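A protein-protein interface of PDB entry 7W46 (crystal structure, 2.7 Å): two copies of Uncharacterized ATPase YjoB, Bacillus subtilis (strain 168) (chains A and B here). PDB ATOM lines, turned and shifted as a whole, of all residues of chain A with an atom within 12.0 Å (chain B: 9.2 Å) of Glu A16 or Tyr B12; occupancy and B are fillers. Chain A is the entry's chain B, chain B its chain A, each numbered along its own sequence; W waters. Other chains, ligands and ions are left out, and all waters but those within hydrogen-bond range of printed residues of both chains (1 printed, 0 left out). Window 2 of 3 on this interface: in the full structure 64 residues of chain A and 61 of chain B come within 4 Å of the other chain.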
ATOM      1  N   TYR A  10     -45.018  13.282  -8.373  1.00  0.00           N
ATOM      2  CA  TYR A  10     -43.696  12.943  -7.856  1.00  0.00           C
ATOM      3  C   TYR A  10     -43.465  13.680  -6.548  1.00  0.00           C
ATOM      4  O   TYR A  10     -43.415  14.913  -6.530  1.00  0.00           O
ATOM      5  CB  TYR A  10     -42.641  13.328  -8.884  1.00  0.00           C
ATOM      6  CG  TYR A  10     -41.202  12.971  -8.619  1.00  0.00           C
ATOM      7  CD1 TYR A  10     -40.685  11.736  -9.017  1.00  0.00           C
ATOM      8  CD2 TYR A  10     -40.326  13.907  -8.083  1.00  0.00           C
ATOM      9  CE1 TYR A  10     -39.328  11.427  -8.842  1.00  0.00           C
ATOM     10  CE2 TYR A  10     -38.978  13.612  -7.899  1.00  0.00           C
ATOM     11  CZ  TYR A  10     -38.481  12.375  -8.278  1.00  0.00           C
ATOM     12  OH  TYR A  10     -37.145  12.088  -8.095  1.00  0.00           O
ATOM     13  N   TYR A  12     -40.835  12.605  -4.321  1.00  0.00           N
ATOM     14  CA  TYR A  12     -39.517  12.280  -3.798  1.00  0.00           C
ATOM     15  C   TYR A  12     -38.780  13.568  -3.467  1.00  0.00           C
ATOM     16  O   TYR A  12     -38.614  14.432  -4.336  1.00  0.00           O
ATOM     17  CB  TYR A  12     -38.743  11.444  -4.817  1.00  0.00           C
ATOM     18  CG  TYR A  12     -37.352  11.053  -4.392  1.00  0.00           C
ATOM     19  CD1 TYR A  12     -37.148  10.063  -3.430  1.00  0.00           C
ATOM     20  CD2 TYR A  12     -36.234  11.669  -4.955  1.00  0.00           C
ATOM     21  CE1 TYR A  12     -35.860   9.702  -3.032  1.00  0.00           C
ATOM     22  CE2 TYR A  12     -34.940  11.322  -4.565  1.00  0.00           C
ATOM     23  CZ  TYR A  12     -34.759  10.334  -3.610  1.00  0.00           C
ATOM     24  OH  TYR A  12     -33.482   9.978  -3.229  1.00  0.00           O
ATOM     25  N   GLU A  13     -38.370  13.714  -2.206  1.00  0.00           N
ATOM     26  CA  GLU A  13     -37.534  14.834  -1.789  1.00  0.00           C
ATOM     27  C   GLU A  13     -36.063  14.470  -1.968  1.00  0.00           C
ATOM     28  O   GLU A  13     -35.599  13.441  -1.463  1.00  0.00           O
ATOM     29  CB  GLU A  13     -37.820  15.224  -0.339  1.00  0.00           C
ATOM     30  CG  GLU A  13     -37.147  16.537   0.081  1.00  0.00           C
ATOM     31  CD  GLU A  13     -37.954  17.779  -0.294  1.00  0.00           C
ATOM     32  OE1 GLU A  13     -38.346  17.926  -1.480  1.00  0.00           O
ATOM     33  OE2 GLU A  13     -38.196  18.609   0.610  1.00  0.00           O
ATOM     34  N   GLU A  14     -35.338  15.330  -2.677  1.00  0.00           N
ATOM     35  CA  GLU A  14     -34.001  15.042  -3.183  1.00  0.00           C
ATOM     36  C   GLU A  14     -32.918  15.375  -2.151  1.00  0.00           C
ATOM     37  O   GLU A  14     -33.031  16.343  -1.390  1.00  0.00           O
ATOM     38  CB  GLU A  14     -33.780  15.824  -4.492  1.00  0.00           C
ATOM     39  CG  GLU A  14     -33.309  17.295  -4.343  1.00  0.00           C
ATOM     40  CD  GLU A  14     -34.390  18.300  -3.847  1.00  0.00           C
ATOM     41  OE1 GLU A  14     -35.458  17.890  -3.323  1.00  0.00           O
ATOM     42  OE2 GLU A  14     -34.121  19.522  -3.927  1.00  0.00           O
ATOM     43  N   LYS A  15     -31.888  14.531  -2.099  1.00  0.00           N
ATOM     44  CA  LYS A  15     -30.718  14.819  -1.280  1.00  0.00           C
ATOM     45  C   LYS A  15     -29.892  15.943  -1.910  1.00  0.00           C
ATOM     46  O   LYS A  15     -30.009  16.251  -3.103  1.00  0.00           O
ATOM     47  CB  LYS A  15     -29.852  13.564  -1.112  1.00  0.00           C
ATOM     48  CG  LYS A  15     -30.623  12.238  -0.993  1.00  0.00           C
ATOM     49  CD  LYS A  15     -31.733  12.294   0.068  1.00  0.00           C
ATOM     50  CE  LYS A  15     -32.876  11.319  -0.243  1.00  0.00           C
ATOM     51  NZ  LYS A  15     -33.608  10.868   0.980  1.00  0.00           N
ATOM     52  N   GLU A  16     -29.038  16.563  -1.097  1.00  0.00           N
ATOM     53  CA  GLU A  16     -28.217  17.640  -1.631  1.00  0.00           C
ATOM     54  C   GLU A  16     -27.251  17.138  -2.697  1.00  0.00           C
ATOM     55  O   GLU A  16     -26.855  17.903  -3.581  1.00  0.00           O
ATOM     56  CB  GLU A  16     -27.448  18.331  -0.510  1.00  0.00           C
ATOM     57  CG  GLU A  16     -26.842  19.660  -0.929  1.00  0.00           C
ATOM     58  CD  GLU A  16     -25.971  20.283   0.153  1.00  0.00           C
ATOM     59  OE1 GLU A  16     -25.377  21.357  -0.116  1.00  0.00           O
ATOM     60  OE2 GLU A  16     -25.885  19.702   1.263  1.00  0.00           O
ATOM     61  N   ASN A  17     -26.879  15.857  -2.647  1.00  0.00           N
ATOM     62  CA  ASN A  17     -25.913  15.333  -3.608  1.00  0.00           C
ATOM     63  C   ASN A  17     -26.519  15.165  -4.994  1.00  0.00           C
ATOM     64  O   ASN A  17     -25.825  15.349  -5.999  1.00  0.00           O
ATOM     65  CB  ASN A  17     -25.345  14.003  -3.109  1.00  0.00           C
ATOM     66  CG  ASN A  17     -24.166  14.198  -2.174  1.00  0.00           C
ATOM     67  OD1 ASN A  17     -23.813  15.334  -1.833  1.00  0.00           O
ATOM     68  ND2 ASN A  17     -23.556  13.091  -1.741  1.00  0.00           N
ATOM     69  N   GLU A  18     -27.803  14.819  -5.082  1.00  0.00           N
ATOM     70  CA  GLU A  18     -28.396  14.614  -6.396  1.00  0.00           C
ATOM     71  C   GLU A  18     -28.413  15.877  -7.248  1.00  0.00           C
ATOM     72  O   GLU A  18     -28.661  15.783  -8.455  1.00  0.00           O
ATOM     73  CB  GLU A  18     -29.817  14.089  -6.259  1.00  0.00           C
ATOM     74  CG  GLU A  18     -29.901  12.647  -5.831  1.00  0.00           C
ATOM     75  CD  GLU A  18     -31.295  12.294  -5.380  1.00  0.00           C
ATOM     76  OE1 GLU A  18     -32.255  12.982  -5.812  1.00  0.00           O
ATOM     77  OE2 GLU A  18     -31.426  11.349  -4.580  1.00  0.00           O
ATOM     78  N   ARG A  19     -28.152  17.045  -6.672  1.00  0.00           N
ATOM     79  CA  ARG A  19     -28.201  18.246  -7.486  1.00  0.00           C
ATOM     80  C   ARG A  19     -26.911  18.501  -8.260  1.00  0.00           C
ATOM     81  O   ARG A  19     -26.878  19.432  -9.073  1.00  0.00           O
ATOM     82  CB  ARG A  19     -28.574  19.456  -6.620  1.00  0.00           C
ATOM     83  CG  ARG A  19     -27.661  19.760  -5.460  1.00  0.00           C
ATOM     84  CD  ARG A  19     -28.259  20.874  -4.594  1.00  0.00           C
ATOM     85  NE  ARG A  19     -29.680  20.641  -4.310  1.00  0.00           N
ATOM     86  CZ  ARG A  19     -30.364  21.229  -3.327  1.00  0.00           C
ATOM     87  NH1 ARG A  19     -29.758  22.095  -2.516  1.00  0.00           N
ATOM     88  NH2 ARG A  19     -31.659  20.950  -3.159  1.00  0.00           N
ATOM     89  N   ALA A  20     -25.874  17.681  -8.081  1.00  0.00           N
ATOM     90  CA  ALA A  20     -24.604  17.918  -8.761  1.00  0.00           C
ATOM     91  C   ALA A  20     -24.754  17.806 -10.275  1.00  0.00           C
ATOM     92  O   ALA A  20     -25.430  16.909 -10.787  1.00  0.00           O
ATOM     93  CB  ALA A  20     -23.540  16.938  -8.272  1.00  0.00           C
ATOM     94  N   ALA A  21     -24.109  18.726 -10.988  1.00  0.00           N
ATOM     95  CA  ALA A  21     -24.219  18.809 -12.436  1.00  0.00           C
ATOM     96  C   ALA A  21     -23.095  18.011 -13.094  1.00  0.00           C
ATOM     97  O   ALA A  21     -21.906  18.283 -12.868  1.00  0.00           O
ATOM     98  CB  ALA A  21     -24.191  20.265 -12.885  1.00  0.00           C
ATOM     99  N   ALA A  22     -23.488  17.038 -13.921  1.00  0.00           N
ATOM    100  CA  ALA A  22     -22.560  16.105 -14.543  1.00  0.00           C
ATOM    101  C   ALA A  22     -21.413  16.820 -15.247  1.00  0.00           C
ATOM    102  O   ALA A  22     -21.628  17.727 -16.057  1.00  0.00           O
ATOM    103  CB  ALA A  22     -23.311  15.225 -15.539  1.00  0.00           C
ATOM    104  N   GLY A  23     -20.188  16.390 -14.946  1.00  0.00           N
ATOM    105  CA  GLY A  23     -19.026  16.892 -15.636  1.00  0.00           C
ATOM    106  C   GLY A  23     -18.615  18.289 -15.258  1.00  0.00           C
ATOM    107  O   GLY A  23     -17.514  18.716 -15.646  1.00  0.00           O
ATOM    108  N   TYR A  24     -19.452  19.016 -14.502  1.00  0.00           N
ATOM    109  CA  TYR A  24     -19.100  20.375 -14.103  1.00  0.00           C
ATOM    110  C   TYR A  24     -17.995  20.387 -13.061  1.00  0.00           C
ATOM    111  O   TYR A  24     -17.207  21.334 -13.011  1.00  0.00           O
ATOM    112  CB  TYR A  24     -20.315  21.125 -13.559  1.00  0.00           C
ATOM    113  CG  TYR A  24     -19.923  22.505 -13.073  1.00  0.00           C
ATOM    114  CD1 TYR A  24     -19.482  23.483 -13.979  1.00  0.00           C
ATOM    115  CD2 TYR A  24     -19.938  22.825 -11.712  1.00  0.00           C
ATOM    116  CE1 TYR A  24     -19.092  24.747 -13.545  1.00  0.00           C
ATOM    117  CE2 TYR A  24     -19.561  24.087 -11.269  1.00  0.00           C
ATOM    118  CZ  TYR A  24     -19.134  25.053 -12.196  1.00  0.00           C
ATOM    119  OH  TYR A  24     -18.746  26.321 -11.772  1.00  0.00           O
ATOM    120  N   GLY A  25     -17.923  19.349 -12.227  1.00  0.00           N
ATOM    121  CA  GLY A  25     -16.898  19.301 -11.196  1.00  0.00           C
ATOM    122  C   GLY A  25     -15.493  19.286 -11.760  1.00  0.00           C
ATOM    123  O   GLY A  25     -14.616  20.012 -11.287  1.00  0.00           O
ATOM    124  N   THR A  26     -15.261  18.466 -12.790  1.00  0.00           N
ATOM    125  CA  THR A  26     -13.976  18.518 -13.478  1.00  0.00           C
ATOM    126  C   THR A  26     -13.794  19.857 -14.200  1.00  0.00           C
ATOM    127  O   THR A  26     -12.793  20.558 -14.010  1.00  0.00           O
ATOM    128  CB  THR A  26     -13.846  17.348 -14.466  1.00  0.00           C
ATOM    129  OG1 THR A  26     -14.234  16.117 -13.841  1.00  0.00           O
ATOM    130  CG2 THR A  26     -12.399  17.221 -14.970  1.00  0.00           C
ATOM    131  N   PHE A  27     -14.753  20.228 -15.040  1.00  0.00           N
ATOM    132  CA  PHE A  27     -14.590  21.424 -15.859  1.00  0.00           C
ATOM    133  C   PHE A  27     -14.306  22.662 -15.009  1.00  0.00           C
ATOM    134  O   PHE A  27     -13.382  23.434 -15.305  1.00  0.00           O
ATOM    135  CB  PHE A  27     -15.838  21.620 -16.708  1.00  0.00           C
ATOM    136  CG  PHE A  27     -15.672  22.631 -17.770  1.00  0.00           C
ATOM    137  CD1 PHE A  27     -15.877  23.976 -17.500  1.00  0.00           C
ATOM    138  CD2 PHE A  27     -15.285  22.248 -19.042  1.00  0.00           C
ATOM    139  CE1 PHE A  27     -15.706  24.921 -18.489  1.00  0.00           C
ATOM    140  CE2 PHE A  27     -15.108  23.186 -20.023  1.00  0.00           C
ATOM    141  CZ  PHE A  27     -15.318  24.534 -19.746  1.00  0.00           C
ATOM    142  N   GLY A  28     -15.093  22.870 -13.944  1.00  0.00           N
ATOM    143  CA  GLY A  28     -14.888  24.043 -13.112  1.00  0.00           C
ATOM    144  C   GLY A  28     -13.532  24.043 -12.430  1.00  0.00           C
ATOM    145  O   GLY A  28     -12.896  25.092 -12.283  1.00  0.00           O
ATOM    146  N   TYR A  29     -13.087  22.871 -11.975  1.00  0.00           N
ATOM    147  CA  TYR A  29     -11.763  22.756 -11.375  1.00  0.00           C
ATOM    148  C   TYR A  29     -10.680  23.161 -12.373  1.00  0.00           C
ATOM    149  O   TYR A  29      -9.835  24.017 -12.072  1.00  0.00           O
ATOM    150  CB  TYR A  29     -11.555  21.325 -10.871  1.00  0.00           C
ATOM    151  CG  TYR A  29     -10.143  20.979 -10.470  1.00  0.00           C
ATOM    152  CD1 TYR A  29      -9.506  21.683  -9.467  1.00  0.00           C
ATOM    153  CD2 TYR A  29      -9.452  19.938 -11.082  1.00  0.00           C
ATOM    154  CE1 TYR A  29      -8.224  21.387  -9.078  1.00  0.00           C
ATOM    155  CE2 TYR A  29      -8.151  19.620 -10.695  1.00  0.00           C
ATOM    156  CZ  TYR A  29      -7.542  20.361  -9.686  1.00  0.00           C
ATOM    157  OH  TYR A  29      -6.257  20.090  -9.269  1.00  0.00           O
ATOM    158  N   THR A  32     -10.742  26.940 -13.137  1.00  0.00           N
ATOM    159  CA  THR A  32     -10.198  27.670 -11.998  1.00  0.00           C
ATOM    160  C   THR A  32      -8.682  27.547 -11.931  1.00  0.00           C
ATOM    161  O   THR A  32      -7.982  28.551 -11.751  1.00  0.00           O
ATOM    162  CB  THR A  32     -10.844  27.146 -10.721  1.00  0.00           C
ATOM    163  OG1 THR A  32     -12.261  27.121 -10.913  1.00  0.00           O
ATOM    164  CG2 THR A  32     -10.470  28.011  -9.508  1.00  0.00           C
ATOM    165  N   PHE B   8     -24.842  33.670  -8.201  1.00  0.00           N
ATOM    166  CA  PHE B   8     -24.700  32.399  -8.899  1.00  0.00           C
ATOM    167  C   PHE B   8     -25.866  31.472  -8.574  1.00  0.00           C
ATOM    168  O   PHE B   8     -26.180  31.220  -7.403  1.00  0.00           O
ATOM    169  CB  PHE B   8     -23.353  31.747  -8.598  1.00  0.00           C
ATOM    170  CG  PHE B   8     -22.207  32.507  -9.179  1.00  0.00           C
ATOM    171  CD1 PHE B   8     -22.109  32.687 -10.548  1.00  0.00           C
ATOM    172  CD2 PHE B   8     -21.253  33.101  -8.358  1.00  0.00           C
ATOM    173  CE1 PHE B   8     -21.062  33.425 -11.094  1.00  0.00           C
ATOM    174  CE2 PHE B   8     -20.199  33.842  -8.904  1.00  0.00           C
ATOM    175  CZ  PHE B   8     -20.109  34.003 -10.267  1.00  0.00           C
ATOM    176  N   ILE B   9     -26.511  30.987  -9.635  1.00  0.00           N
ATOM    177  CA  ILE B   9     -27.662  30.103  -9.508  1.00  0.00           C
ATOM    178  C   ILE B   9     -27.247  28.794  -8.864  1.00  0.00           C
ATOM    179  O   ILE B   9     -27.923  28.277  -7.965  1.00  0.00           O
ATOM    180  CB  ILE B   9     -28.294  29.877 -10.893  1.00  0.00           C
ATOM    181  CG1 ILE B   9     -28.798  31.205 -11.475  1.00  0.00           C
ATOM    182  CG2 ILE B   9     -29.372  28.812 -10.854  1.00  0.00           C
ATOM    183  CD1 ILE B   9     -29.729  31.982 -10.585  1.00  0.00           C
ATOM    184  N   TYR B  10     -26.135  28.233  -9.332  1.00  0.00           N
ATOM    185  CA  TYR B  10     -25.614  26.958  -8.855  1.00  0.00           C
ATOM    186  C   TYR B  10     -24.676  27.227  -7.684  1.00  0.00           C
ATOM    187  O   TYR B  10     -23.640  27.875  -7.846  1.00  0.00           O
ATOM    188  CB  TYR B  10     -24.896  26.240  -9.991  1.00  0.00           C
ATOM    189  CG  TYR B  10     -24.490  24.815  -9.706  1.00  0.00           C
ATOM    190  CD1 TYR B  10     -25.429  23.788  -9.727  1.00  0.00           C
ATOM    191  CD2 TYR B  10     -23.156  24.491  -9.446  1.00  0.00           C
ATOM    192  CE1 TYR B  10     -25.054  22.475  -9.492  1.00  0.00           C
ATOM    193  CE2 TYR B  10     -22.772  23.192  -9.208  1.00  0.00           C
ATOM    194  CZ  TYR B  10     -23.725  22.180  -9.232  1.00  0.00           C
ATOM    195  OH  TYR B  10     -23.357  20.873  -8.994  1.00  0.00           O
ATOM    196  N   GLN B  11     -25.043  26.730  -6.507  1.00  0.00           N
ATOM    197  CA  GLN B  11     -24.302  26.982  -5.283  1.00  0.00           C
ATOM    198  C   GLN B  11     -23.802  25.712  -4.618  1.00  0.00           C
ATOM    199  O   GLN B  11     -23.182  25.791  -3.561  1.00  0.00           O
ATOM    200  CB  GLN B  11     -25.170  27.759  -4.290  1.00  0.00           C
ATOM    201  CG  GLN B  11     -25.676  29.059  -4.804  1.00  0.00           C
ATOM    202  CD  GLN B  11     -26.048  30.008  -3.696  1.00  0.00           C
ATOM    203  OE1 GLN B  11     -25.385  31.036  -3.500  1.00  0.00           O
ATOM    204  NE2 GLN B  11     -27.127  29.681  -2.962  1.00  0.00           N
ATOM    205  N   TYR B  12     -24.088  24.548  -5.185  1.00  0.00           N
ATOM    206  CA  TYR B  12     -23.509  23.306  -4.701  1.00  0.00           C
ATOM    207  C   TYR B  12     -21.989  23.372  -4.800  1.00  0.00           C
ATOM    208  O   TYR B  12     -21.437  23.732  -5.844  1.00  0.00           O
ATOM    209  CB  TYR B  12     -24.059  22.148  -5.530  1.00  0.00           C
ATOM    210  CG  TYR B  12     -23.626  20.759  -5.120  1.00  0.00           C
ATOM    211  CD1 TYR B  12     -24.254  20.093  -4.064  1.00  0.00           C
ATOM    212  CD2 TYR B  12     -22.614  20.087  -5.814  1.00  0.00           C
ATOM    213  CE1 TYR B  12     -23.870  18.801  -3.701  1.00  0.00           C
ATOM    214  CE2 TYR B  12     -22.226  18.796  -5.458  1.00  0.00           C
ATOM    215  CZ  TYR B  12     -22.859  18.158  -4.403  1.00  0.00           C
ATOM    216  OH  TYR B  12     -22.481  16.881  -4.046  1.00  0.00           O
ATOM    217  N   GLU B  13     -21.309  23.070  -3.699  1.00  0.00           N
ATOM    218  CA  GLU B  13     -19.865  22.884  -3.726  1.00  0.00           C
ATOM    219  C   GLU B  13     -19.576  21.421  -3.445  1.00  0.00           C
ATOM    220  O   GLU B  13     -20.193  20.812  -2.564  1.00  0.00           O
ATOM    221  CB  GLU B  13     -19.143  23.785  -2.719  1.00  0.00           C
ATOM    222  CG  GLU B  13     -17.703  24.112  -3.127  1.00  0.00           C
ATOM    223  CD  GLU B  13     -17.608  24.937  -4.419  1.00  0.00           C
ATOM    224  OE1 GLU B  13     -18.146  26.069  -4.445  1.00  0.00           O
ATOM    225  OE2 GLU B  13     -16.992  24.458  -5.408  1.00  0.00           O
ATOM    226  N   GLU B  14     -18.667  20.846  -4.215  1.00  0.00           N
ATOM    227  CA  GLU B  14     -18.536  19.403  -4.230  1.00  0.00           C
ATOM    228  C   GLU B  14     -17.211  18.937  -3.642  1.00  0.00           C
ATOM    229  O   GLU B  14     -16.204  19.656  -3.662  1.00  0.00           O
ATOM    230  CB  GLU B  14     -18.679  18.861  -5.647  1.00  0.00           C
ATOM    231  CG  GLU B  14     -19.132  17.423  -5.655  1.00  0.00           C
ATOM    232  CD  GLU B  14     -19.528  16.950  -7.024  1.00  0.00           C
ATOM    233  OE1 GLU B  14     -18.961  17.475  -8.014  1.00  0.00           O
ATOM    234  OE2 GLU B  14     -20.373  16.027  -7.106  1.00  0.00           O
ATOM    235  N   LYS B  15     -17.245  17.711  -3.113  1.00  0.00           N
ATOM    236  CA  LYS B  15     -16.044  17.020  -2.665  1.00  0.00           C
ATOM    237  C   LYS B  15     -15.077  16.818  -3.831  1.00  0.00           C
ATOM    238  O   LYS B  15     -15.481  16.652  -4.988  1.00  0.00           O
ATOM    239  CB  LYS B  15     -16.416  15.672  -2.047  1.00  0.00           C
ATOM    240  CG  LYS B  15     -17.659  15.705  -1.169  1.00  0.00           C
ATOM    241  CD  LYS B  15     -17.393  16.450   0.134  1.00  0.00           C
ATOM    242  CE  LYS B  15     -18.462  16.128   1.160  1.00  0.00           C
ATOM    243  NZ  LYS B  15     -18.935  14.726   1.007  1.00  0.00           N
ATOM    244  N   GLU B  16     -13.781  16.823  -3.517  1.00  0.00           N
ATOM    245  CA  GLU B  16     -12.800  16.762  -4.590  1.00  0.00           C
ATOM    246  C   GLU B  16     -12.722  15.400  -5.258  1.00  0.00           C
ATOM    247  O   GLU B  16     -12.125  15.306  -6.334  1.00  0.00           O
ATOM    248  CB  GLU B  16     -11.420  17.163  -4.085  1.00  0.00           C
ATOM    249  CG  GLU B  16     -10.874  16.300  -2.976  1.00  0.00           C
ATOM    250  CD  GLU B  16      -9.586  16.865  -2.414  1.00  0.00           C
ATOM    251  OE1 GLU B  16      -8.593  16.110  -2.329  1.00  0.00           O
ATOM    252  OE2 GLU B  16      -9.564  18.074  -2.077  1.00  0.00           O
ATOM    253  N   ASN B  17     -13.306  14.347  -4.675  1.00  0.00           N
ATOM    254  CA  ASN B  17     -13.363  13.079  -5.401  1.00  0.00           C
ATOM    255  C   ASN B  17     -14.180  13.207  -6.680  1.00  0.00           C
ATOM    256  O   ASN B  17     -14.052  12.362  -7.572  1.00  0.00           O
ATOM    257  CB  ASN B  17     -13.927  11.947  -4.526  1.00  0.00           C
ATOM    258  CG  ASN B  17     -15.133  12.368  -3.691  1.00  0.00           C
ATOM    259  OD1 ASN B  17     -15.824  13.339  -4.004  1.00  0.00           O
ATOM    260  ND2 ASN B  17     -15.386  11.629  -2.615  1.00  0.00           N
ATOM    261  N   GLU B  18     -14.978  14.268  -6.801  1.00  0.00           N
ATOM    262  CA  GLU B  18     -15.857  14.473  -7.943  1.00  0.00           C
ATOM    263  C   GLU B  18     -15.285  15.459  -8.951  1.00  0.00           C
ATOM    264  O   GLU B  18     -15.946  15.774  -9.948  1.00  0.00           O
ATOM    265  CB  GLU B  18     -17.228  14.938  -7.481  1.00  0.00           C
ATOM    266  CG  GLU B  18     -17.850  14.166  -6.294  1.00  0.00           C
ATOM    267  CD  GLU B  18     -18.144  12.670  -6.548  1.00  0.00           C
ATOM    268  OE1 GLU B  18     -18.055  12.206  -7.710  1.00  0.00           O
ATOM    269  OE2 GLU B  18     -18.477  11.953  -5.569  1.00  0.00           O
HETATM  270  O   HOH W   1     -16.987  16.474 -12.805  1.00  0.00           O
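The side-chain carboxylate (OE2) of Glu B18 lies close to the side-chain amide oxygen (OD1) of Asn B17, at 3.4 Å.
OE2 of Glu A14 is in salt-bridge range of NH2 of Arg A19 (2.9 Å).
Glu A16 touches one residue of chain B.
Of chain A, only Glu A16 (3.1 Å), Asn A17 (3.0 Å), Arg A19 (3.7 Å) and Ala A20 (3.6 Å) come within 4 Å of Tyr B12.
Of chain A, only Arg A19, Ala A20, Ala A21 and Tyr A24 come within 4 Å of Tyr B10.
No residue of chain A comes within 4 Å of Gln B11.
No residue of chain A comes within 4 Å of Glu B13.
Of chain A, only Ala A20 comes within 4 Å of Glu B14.
No residue of chain A comes within 4 Å of Lys B15.
Of the printed residues of chain B, Gly A25 touches Glu B18 (3.9 Å).
Printed residues of chain B within 4 Å of Arg A19: Tyr B10 and Tyr B12.
Glu A18 touches none of the printed residues of chain B.
The nearest residue of chain B that does not touch Glu A16 is Glu B13 (5.7 Å).
Printed residues of chain A that touch a printed residue of chain B: Glu A16, Asn A17, Arg A19, Ala A20, Ala A21, Tyr A24, Gly A25 and Thr A26.
Hydrophobic or aromatic side chains of chain A that line the printed part of chain B: Ala A20 and Tyr A24.
Of the 11 printed residues of chain B, 4 touch a printed residue of chain A.
Printed residues of chain B that touch a printed residue of chain A: Tyr B10, Tyr B12, Glu B14 and Glu B18.
Hydrophobic or aromatic side chains of chain B within 4 Å of the printed part of chain A: Tyr B10 and Tyr B12.
Glu A16 touches Tyr B12, but with the chains exchanged Tyr A12 does not touch Glu B16 (20.9 Å).
Asn A17 touches Tyr B12, but with the chains exchanged Tyr A12 does not touch Asn B17 (18.0 Å).
8 positions are printed for both chains.
Of the 11 pairs that touch across the chains among the printed residues, none has its exchanged pair printed and touching as well.
Water W1 lies within hydrogen-bond range of the backbone NH of Thr A26 (2.6 Å), the backbone NH of Gly A25 (3.1 Å) and the backbone carbonyl oxygen of Glu B18 (3.1 Å).
The side-chain hydroxyl (OH) of Tyr B10 is in hydrogen-bond range of the backbone NH (N) of Ala A21, at 3.0 Å.
The side-chain hydroxyl of Tyr B12 sits at hydrogen-bond distance from the side-chain amide oxygen of Asn A17, at 3.0 Å.
O of Glu A16 touches CE1 of Tyr B12, 3.1 Å away.
Arg A19 touches Tyr B10.
Arg A19 touches Tyr B12.
Ala A20 touches Tyr B10 (CA to OH, 3.2 Å).
CB of Ala A20 touches CE2 of Tyr B12, at 3.6 Å.
OE2 of Glu B14 touches CB of Ala A20 (3.5 Å).
Tyr B10 touches Tyr A24 (CE2 to CD2, 3.8 Å).
Gly A25 touches Glu B18 (CA to O, 3.9 Å).
Glu B18 touches Thr A26 (O to N, 3.97 Å).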
